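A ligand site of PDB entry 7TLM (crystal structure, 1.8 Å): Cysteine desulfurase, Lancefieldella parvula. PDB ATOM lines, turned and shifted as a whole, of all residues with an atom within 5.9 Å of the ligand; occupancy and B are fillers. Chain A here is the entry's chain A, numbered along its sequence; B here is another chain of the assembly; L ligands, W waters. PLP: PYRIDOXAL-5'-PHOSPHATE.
N of Glu 123 sits at hydrogen-bond distance from OD1 of Asn 120 (2.8 Å). The backbone carbonyl oxygen of Val 200 lies within hydrogen-bond range of the side-chain hydroxyl of Thr 198, 2.8 Å away. The side-chain amide nitrogen (ND2) of Asn 120 sits at hydrogen-bond distance from the backbone carbonyl oxygen (O) of Ala 302 of chain B, at 3.1 Å. A ring nitrogen (ND1) of His 150 lies within hydrogen-bond range of the backbone NH (N) of Ser 152, 2.9 Å away. The side-chain carboxylate (OD1) of Asp 227 is in hydrogen-bond range of the backbone NH (N) of Ala 229. OG of Ser 250 is in hydrogen-bond range of OG1 of Thr 121, 2.7 Å away. NE2 of His 252 sits close to OG1 of Thr 304 of chain B (3.3 Å). N of Ser 122 sits close to OD1 of Asn 120 (3.3 Å).
Water W1 lies within hydrogen-bond range of an oxygen (O1P) of the ligand (2.8 Å) and a ring nitrogen (NE2) of His 150 (3.3 Å).
Asn 120 touches the ligand (CB to O3P, 3.2 Å). Thr 121 touches the ligand. His 150 touches the ligand (CD2 to C4, 3.5 Å). OG1 of Thr 198 touches C2A of the ligand, 3.8 Å away. Val 200 touches the ligand. CB of Asn 202 touches O3 of the ligand, 3.3 Å away. CB of Ala 229 touches C2 of the ligand, 3.5 Å away. Gly 303 of chain B touches the ligand. Hydrophobic or aromatic side chains within 4 Å of the ligand: His 150, Ala 229 and His 252.
C4A of the ligand is covalently linked to NZ of Lys 253, at 1.4 Å. An oxygen (O1P) of the ligand lies within hydrogen-bond range of the side-chain hydroxyl (OG1) of Thr 304 of chain B. An oxygen (O1P) of the ligand is in hydrogen-bond range of the backbone NH (N) of Thr 304 of chain B (2.8 Å). NE2 of His 252 is in hydrogen-bond range of O2P of the ligand, at 2.7 Å. The side-chain hydroxyl of Ser 250 is in hydrogen-bond range of an oxygen (O2P) of the ligand, 2.5 Å away. O3P of the ligand lies within hydrogen-bond range of OG of Ser 122. The side-chain carboxylate (OD2) of Asp 227 lies within hydrogen-bond range of a nitrogen (N1) of the ligand (2.6 Å). N of Ser 122 lies within hydrogen-bond range of O3P of the ligand (2.9 Å).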
ATOM      1  N   ALA A  51      -7.824  14.442  37.119  1.00  0.00           N
ATOM      2  CA  ALA A  51      -8.934  14.018  36.276  1.00  0.00           C
ATOM      3  C   ALA A  51      -8.482  13.710  34.858  1.00  0.00           C
ATOM      4  O   ALA A  51      -9.185  13.005  34.117  1.00  0.00           O
ATOM      5  CB  ALA A  51     -10.031  15.097  36.284  1.00  0.00           C
ATOM      6  N   ALA A  52      -7.335  14.252  34.447  1.00  0.00           N
ATOM      7  CA  ALA A  52      -6.752  13.877  33.153  1.00  0.00           C
ATOM      8  C   ALA A  52      -5.923  12.608  33.278  1.00  0.00           C
ATOM      9  O   ALA A  52      -6.115  11.665  32.519  1.00  0.00           O
ATOM     10  CB  ALA A  52      -5.904  15.023  32.601  1.00  0.00           C
ATOM     11  N   ARG A 119      -6.908  -0.854  25.876  1.00  0.00           N
ATOM     12  CA  ARG A 119      -5.903   0.194  26.099  1.00  0.00           C
ATOM     13  C   ARG A 119      -6.397   1.266  27.068  1.00  0.00           C
ATOM     14  O   ARG A 119      -5.590   1.820  27.810  1.00  0.00           O
ATOM     15  CB  ARG A 119      -5.527   0.856  24.764  1.00  0.00           C
ATOM     16  CG  ARG A 119      -4.713   2.182  24.876  1.00  0.00           C
ATOM     17  CD  ARG A 119      -4.399   2.811  23.479  1.00  0.00           C
ATOM     18  NE  ARG A 119      -5.499   2.593  22.553  1.00  0.00           N
ATOM     19  CZ  ARG A 119      -5.541   1.618  21.646  1.00  0.00           C
ATOM     20  NH1 ARG A 119      -4.509   0.794  21.501  1.00  0.00           N
ATOM     21  NH2 ARG A 119      -6.625   1.472  20.890  1.00  0.00           N
ATOM     22  N   ASN A 120      -7.698   1.553  27.062  1.00  0.00           N
ATOM     23  CA  ASN A 120      -8.284   2.635  27.837  1.00  0.00           C
ATOM     24  C   ASN A 120      -9.800   2.510  27.834  1.00  0.00           C
ATOM     25  O   ASN A 120     -10.372   1.662  27.129  1.00  0.00           O
ATOM     26  CB  ASN A 120      -7.805   4.005  27.310  1.00  0.00           C
ATOM     27  CG  ASN A 120      -7.989   4.157  25.800  1.00  0.00           C
ATOM     28  OD1 ASN A 120      -8.855   3.526  25.200  1.00  0.00           O
ATOM     29  ND2 ASN A 120      -7.182   5.041  25.196  1.00  0.00           N
ATOM     30  N   THR A 121     -10.458   3.332  28.661  1.00  0.00           N
ATOM     31  CA  THR A 121     -11.914   3.403  28.631  1.00  0.00           C
ATOM     32  C   THR A 121     -12.429   3.614  27.219  1.00  0.00           C
ATOM     33  O   THR A 121     -13.447   3.027  26.828  1.00  0.00           O
ATOM     34  CB  THR A 121     -12.428   4.541  29.537  1.00  0.00           C
ATOM     35  OG1 THR A 121     -11.970   4.325  30.877  1.00  0.00           O
ATOM     36  CG2 THR A 121     -13.971   4.605  29.529  1.00  0.00           C
ATOM     37  N   SER A 122     -11.754   4.453  26.427  1.00  0.00           N
ATOM     38  CA  SER A 122     -12.253   4.755  25.090  1.00  0.00           C
ATOM     39  C   SER A 122     -12.384   3.497  24.250  1.00  0.00           C
ATOM     40  O   SER A 122     -13.403   3.285  23.586  1.00  0.00           O
ATOM     41  CB  SER A 122     -11.359   5.771  24.391  1.00  0.00           C
ATOM     42  OG  SER A 122     -11.272   6.998  25.126  1.00  0.00           O
ATOM     43  N   GLU A 123     -11.362   2.630  24.275  1.00  0.00           N
ATOM     44  CA  GLU A 123     -11.458   1.405  23.482  1.00  0.00           C
ATOM     45  C   GLU A 123     -12.555   0.492  24.031  1.00  0.00           C
ATOM     46  O   GLU A 123     -13.281  -0.135  23.255  1.00  0.00           O
ATOM     47  CB  GLU A 123     -10.119   0.654  23.433  1.00  0.00           C
ATOM     48  CG  GLU A 123     -10.226  -0.635  22.610  1.00  0.00           C
ATOM     49  CD  GLU A 123      -8.943  -1.416  22.564  1.00  0.00           C
ATOM     50  OE1 GLU A 123      -8.072  -1.156  23.425  1.00  0.00           O
ATOM     51  OE2 GLU A 123      -8.825  -2.336  21.714  1.00  0.00           O
ATOM     52  N   LEU A 125     -15.346   1.379  25.410  1.00  0.00           N
ATOM     53  CA  LEU A 125     -16.645   1.873  24.971  1.00  0.00           C
ATOM     54  C   LEU A 125     -16.846   1.654  23.478  1.00  0.00           C
ATOM     55  O   LEU A 125     -17.979   1.399  23.043  1.00  0.00           O
ATOM     56  CB  LEU A 125     -16.803   3.350  25.347  1.00  0.00           C
ATOM     57  CG  LEU A 125     -16.817   3.632  26.867  1.00  0.00           C
ATOM     58  CD1 LEU A 125     -16.755   5.151  27.152  1.00  0.00           C
ATOM     59  CD2 LEU A 125     -18.087   3.049  27.450  1.00  0.00           C
ATOM     60  N   HIS A 150     -18.390  12.087  28.233  1.00  0.00           N
ATOM     61  CA  HIS A 150     -17.132  12.311  27.555  1.00  0.00           C
ATOM     62  C   HIS A 150     -17.287  11.845  26.094  1.00  0.00           C
ATOM     63  O   HIS A 150     -18.143  11.014  25.774  1.00  0.00           O
ATOM     64  CB  HIS A 150     -16.041  11.545  28.345  1.00  0.00           C
ATOM     65  CG  HIS A 150     -14.665  11.540  27.757  1.00  0.00           C
ATOM     66  ND1 HIS A 150     -14.334  10.856  26.604  1.00  0.00           N
ATOM     67  CD2 HIS A 150     -13.513  12.084  28.219  1.00  0.00           C
ATOM     68  CE1 HIS A 150     -13.040  11.019  26.360  1.00  0.00           C
ATOM     69  NE2 HIS A 150     -12.521  11.765  27.317  1.00  0.00           N
ATOM     70  N   SER A 152     -15.791   9.835  24.313  1.00  0.00           N
ATOM     71  CA  SER A 152     -15.667   8.406  24.075  1.00  0.00           C
ATOM     72  C   SER A 152     -16.930   7.647  24.425  1.00  0.00           C
ATOM     73  O   SER A 152     -17.107   6.499  23.970  1.00  0.00           O
ATOM     74  CB  SER A 152     -14.476   7.857  24.858  1.00  0.00           C
ATOM     75  OG  SER A 152     -13.266   8.403  24.347  1.00  0.00           O
ATOM     76  N   ASN A 153     -17.842   8.250  25.203  1.00  0.00           N
ATOM     77  CA  ASN A 153     -19.160   7.672  25.427  1.00  0.00           C
ATOM     78  C   ASN A 153     -20.233   8.422  24.634  1.00  0.00           C
ATOM     79  O   ASN A 153     -21.403   8.418  25.019  1.00  0.00           O
ATOM     80  CB  ASN A 153     -19.514   7.642  26.922  1.00  0.00           C
ATOM     81  CG  ASN A 153     -20.517   6.556  27.261  1.00  0.00           C
ATOM     82  OD1 ASN A 153     -20.644   5.552  26.548  1.00  0.00           O
ATOM     83  ND2 ASN A 153     -21.231   6.739  28.383  1.00  0.00           N
ATOM     84  N   THR A 198     -22.370   8.159  32.274  1.00  0.00           N
ATOM     85  CA  THR A 198     -21.189   8.306  33.110  1.00  0.00           C
ATOM     86  C   THR A 198     -21.558   8.207  34.588  1.00  0.00           C
ATOM     87  O   THR A 198     -22.573   8.763  35.041  1.00  0.00           O
ATOM     88  CB  THR A 198     -20.485   9.643  32.818  1.00  0.00           C
ATOM     89  OG1 THR A 198     -19.247   9.697  33.526  1.00  0.00           O
ATOM     90  CG2 THR A 198     -21.342  10.851  33.237  1.00  0.00           C
ATOM     91  N   VAL A 200     -19.592   9.404  37.008  1.00  0.00           N
ATOM     92  CA  VAL A 200     -19.187  10.715  37.498  1.00  0.00           C
ATOM     93  C   VAL A 200     -18.700  11.531  36.314  1.00  0.00           C
ATOM     94  O   VAL A 200     -17.837  11.074  35.556  1.00  0.00           O
ATOM     95  CB  VAL A 200     -18.075  10.618  38.576  1.00  0.00           C
ATOM     96  CG1 VAL A 200     -17.579  12.019  38.977  1.00  0.00           C
ATOM     97  CG2 VAL A 200     -18.586   9.858  39.809  1.00  0.00           C
ATOM     98  N   SER A 201     -19.231  12.738  36.152  1.00  0.00           N
ATOM     99  CA  SER A 201     -18.808  13.640  35.076  1.00  0.00           C
ATOM    100  C   SER A 201     -17.380  14.151  35.279  1.00  0.00           C
ATOM    101  O   SER A 201     -17.042  14.645  36.364  1.00  0.00           O
ATOM    102  CB  SER A 201     -19.769  14.819  34.989  1.00  0.00           C
ATOM    103  OG  SER A 201     -19.191  15.883  34.253  1.00  0.00           O
ATOM    104  N   ASN A 202     -16.569  14.114  34.222  1.00  0.00           N
ATOM    105  CA  ASN A 202     -15.178  14.571  34.320  1.00  0.00           C
ATOM    106  C   ASN A 202     -15.077  16.093  34.316  1.00  0.00           C
ATOM    107  O   ASN A 202     -13.973  16.624  34.459  1.00  0.00           O
ATOM    108  CB  ASN A 202     -14.335  14.009  33.155  1.00  0.00           C
ATOM    109  CG  ASN A 202     -14.804  14.509  31.785  1.00  0.00           C
ATOM    110  OD1 ASN A 202     -15.993  14.561  31.500  1.00  0.00           O
ATOM    111  ND2 ASN A 202     -13.838  14.778  30.900  1.00  0.00           N
ATOM    112  N   ASP A 227     -19.908   4.288  32.147  1.00  0.00           N
ATOM    113  CA  ASP A 227     -18.578   4.865  32.013  1.00  0.00           C
ATOM    114  C   ASP A 227     -18.116   5.229  33.422  1.00  0.00           C
ATOM    115  O   ASP A 227     -18.557   6.226  33.993  1.00  0.00           O
ATOM    116  CB  ASP A 227     -18.609   6.073  31.078  1.00  0.00           C
ATOM    117  CG  ASP A 227     -17.251   6.741  30.911  1.00  0.00           C
ATOM    118  OD1 ASP A 227     -16.291   6.418  31.653  1.00  0.00           O
ATOM    119  OD2 ASP A 227     -17.148   7.615  30.025  1.00  0.00           O
ATOM    120  N   ALA A 228     -17.242   4.412  33.992  1.00  0.00           N
ATOM    121  CA  ALA A 228     -16.792   4.609  35.358  1.00  0.00           C
ATOM    122  C   ALA A 228     -15.384   5.210  35.412  1.00  0.00           C
ATOM    123  O   ALA A 228     -14.687   5.078  36.438  1.00  0.00           O
ATOM    124  CB  ALA A 228     -16.852   3.278  36.121  1.00  0.00           C
ATOM    125  N   ALA A 229     -14.940   5.886  34.354  1.00  0.00           N
ATOM    126  CA  ALA A 229     -13.555   6.343  34.333  1.00  0.00           C
ATOM    127  C   ALA A 229     -13.254   7.344  35.445  1.00  0.00           C
ATOM    128  O   ALA A 229     -12.110   7.417  35.924  1.00  0.00           O
ATOM    129  CB  ALA A 229     -13.191   6.958  32.982  1.00  0.00           C
ATOM    130  N   GLN A 230     -14.246   8.143  35.835  1.00  0.00           N
ATOM    131  CA  GLN A 230     -14.071   9.160  36.867  1.00  0.00           C
ATOM    132  C   GLN A 230     -14.612   8.716  38.229  1.00  0.00           C
ATOM    133  O   GLN A 230     -14.386   9.406  39.228  1.00  0.00           O
ATOM    134  CB  GLN A 230     -14.761  10.460  36.435  1.00  0.00           C
ATOM    135  CG  GLN A 230     -14.632  11.673  37.358  1.00  0.00           C
ATOM    136  CD  GLN A 230     -13.250  12.291  37.444  1.00  0.00           C
ATOM    137  OE1 GLN A 230     -12.298  11.841  36.807  1.00  0.00           O
ATOM    138  NE2 GLN A 230     -13.136  13.311  38.279  1.00  0.00           N
ATOM    139  N   SER A 250     -10.351   3.355  33.220  1.00  0.00           N
ATOM    140  CA  SER A 250      -8.948   3.456  32.811  1.00  0.00           C
ATOM    141  C   SER A 250      -8.017   3.356  34.015  1.00  0.00           C
ATOM    142  O   SER A 250      -8.149   4.107  34.987  1.00  0.00           O
ATOM    143  CB  SER A 250      -8.680   4.768  32.078  1.00  0.00           C
ATOM    144  OG  SER A 250      -9.296   4.813  30.806  1.00  0.00           O
ATOM    145  N   HIS A 252      -5.002   4.409  34.269  1.00  0.00           N
ATOM    146  CA  HIS A 252      -4.138   5.563  34.437  1.00  0.00           C
ATOM    147  C   HIS A 252      -4.811   6.694  35.212  1.00  0.00           C
ATOM    148  O   HIS A 252      -4.119   7.617  35.632  1.00  0.00           O
ATOM    149  CB  HIS A 252      -3.630   6.065  33.068  1.00  0.00           C
ATOM    150  CG  HIS A 252      -4.691   6.700  32.205  1.00  0.00           C
ATOM    151  ND1 HIS A 252      -4.996   8.047  32.273  1.00  0.00           N
ATOM    152  CD2 HIS A 252      -5.530   6.171  31.284  1.00  0.00           C
ATOM    153  CE1 HIS A 252      -5.982   8.315  31.429  1.00  0.00           C
ATOM    154  NE2 HIS A 252      -6.319   7.195  30.818  1.00  0.00           N
ATOM    155  N   LYS A 253      -6.128   6.635  35.432  1.00  0.00           N
ATOM    156  CA  LYS A 253      -6.815   7.602  36.282  1.00  0.00           C
ATOM    157  C   LYS A 253      -6.923   7.147  37.728  1.00  0.00           C
ATOM    158  O   LYS A 253      -7.399   7.912  38.585  1.00  0.00           O
ATOM    159  CB  LYS A 253      -8.205   7.918  35.726  1.00  0.00           C
ATOM    160  CG  LYS A 253      -8.134   8.886  34.556  1.00  0.00           C
ATOM    161  CD  LYS A 253      -9.453   9.037  33.860  1.00  0.00           C
ATOM    162  CE  LYS A 253      -9.271   9.765  32.511  1.00  0.00           C
ATOM    163  NZ  LYS A 253     -10.568   9.961  31.833  1.00  0.00           N
ATOM    164  N   ARG A 408     -10.287  23.650  34.478  1.00  0.00           N
ATOM    165  CA  ARG A 408     -10.698  22.527  35.319  1.00  0.00           C
ATOM    166  C   ARG A 408      -9.579  22.172  36.263  1.00  0.00           C
ATOM    167  O   ARG A 408      -8.488  21.830  35.811  1.00  0.00           O
ATOM    168  CB  ARG A 408     -11.092  21.292  34.516  1.00  0.00           C
ATOM    169  CG  ARG A 408     -11.725  20.182  35.393  1.00  0.00           C
ATOM    170  CD  ARG A 408     -11.798  18.887  34.600  1.00  0.00           C
ATOM    171  NE  ARG A 408     -10.474  18.384  34.218  1.00  0.00           N
ATOM    172  CZ  ARG A 408     -10.280  17.321  33.460  1.00  0.00           C
ATOM    173  NH1 ARG A 408     -11.324  16.666  32.962  1.00  0.00           N
ATOM    174  NH2 ARG A 408      -9.045  16.946  33.142  1.00  0.00           N
ATOM    175  N   GLU B 281      -9.849  12.784  21.702  1.00  0.00           N
ATOM    176  CA  GLU B 281      -8.484  12.963  21.223  1.00  0.00           C
ATOM    177  C   GLU B 281      -8.360  12.747  19.704  1.00  0.00           C
ATOM    178  O   GLU B 281      -7.381  13.172  19.096  1.00  0.00           O
ATOM    179  CB  GLU B 281      -7.524  12.014  21.947  1.00  0.00           C
ATOM    180  CG  GLU B 281      -7.453  12.237  23.472  1.00  0.00           C
ATOM    181  CD  GLU B 281      -6.062  12.060  24.048  1.00  0.00           C
ATOM    182  OE1 GLU B 281      -5.920  12.189  25.273  1.00  0.00           O
ATOM    183  OE2 GLU B 281      -5.113  11.777  23.277  1.00  0.00           O
ATOM    184  N   ALA B 302      -7.570   6.902  19.605  1.00  0.00           N
ATOM    185  CA  ALA B 302      -8.721   7.286  20.423  1.00  0.00           C
ATOM    186  C   ALA B 302      -8.341   7.168  21.896  1.00  0.00           C
ATOM    187  O   ALA B 302      -7.812   6.151  22.329  1.00  0.00           O
ATOM    188  CB  ALA B 302      -9.940   6.397  20.135  1.00  0.00           C
ATOM    189  N   GLY B 303      -8.631   8.221  22.665  1.00  0.00           N
ATOM    190  CA  GLY B 303      -8.371   8.245  24.104  1.00  0.00           C
ATOM    191  C   GLY B 303      -6.893   8.368  24.485  1.00  0.00           C
ATOM    192  O   GLY B 303      -5.998   8.574  23.658  1.00  0.00           O
ATOM    193  N   THR B 304      -6.652   8.245  25.785  1.00  0.00           N
ATOM    194  CA  THR B 304      -5.312   8.385  26.343  1.00  0.00           C
ATOM    195  C   THR B 304      -4.374   7.303  25.809  1.00  0.00           C
ATOM    196  O   THR B 304      -4.628   6.108  25.994  1.00  0.00           O
ATOM    197  CB  THR B 304      -5.356   8.327  27.866  1.00  0.00           C
ATOM    198  OG1 THR B 304      -6.163   9.400  28.359  1.00  0.00           O
ATOM    199  CG2 THR B 304      -3.955   8.452  28.473  1.00  0.00           C
HETATM  200  N1  PLP L   1     -14.929   8.874  30.321  1.00  0.00           N
HETATM  201  C2  PLP L   1     -14.621   9.728  31.364  1.00  0.00           C
HETATM  202  C2A PLP L   1     -15.703  10.116  32.344  1.00  0.00           C
HETATM  203  C3  PLP L   1     -13.334  10.242  31.499  1.00  0.00           C
HETATM  204  O3  PLP L   1     -13.046  11.085  32.533  1.00  0.00           O
HETATM  205  C4  PLP L   1     -12.328   9.880  30.605  1.00  0.00           C
HETATM  206  C4A PLP L   1     -11.012  10.592  30.621  1.00  0.00           C
HETATM  207  C5  PLP L   1     -12.637   9.013  29.557  1.00  0.00           C
HETATM  208  C6  PLP L   1     -13.922   8.522  29.423  1.00  0.00           C
HETATM  209  C5A PLP L   1     -11.561   8.619  28.556  1.00  0.00           C
HETATM  210  O4P PLP L   1     -10.556   7.844  29.162  1.00  0.00           O
HETATM  211  P   PLP L   1      -9.314   7.331  28.280  1.00  0.00           P
HETATM  212  O1P PLP L   1      -8.636   8.568  27.708  1.00  0.00           O
HETATM  213  O2P PLP L   1      -8.418   6.617  29.248  1.00  0.00           O
HETATM  214  O3P PLP L   1      -9.857   6.467  27.171  1.00  0.00           O
HETATM  215  O   HOH W   1      -9.569  10.785  26.295  1.00  0.00           O
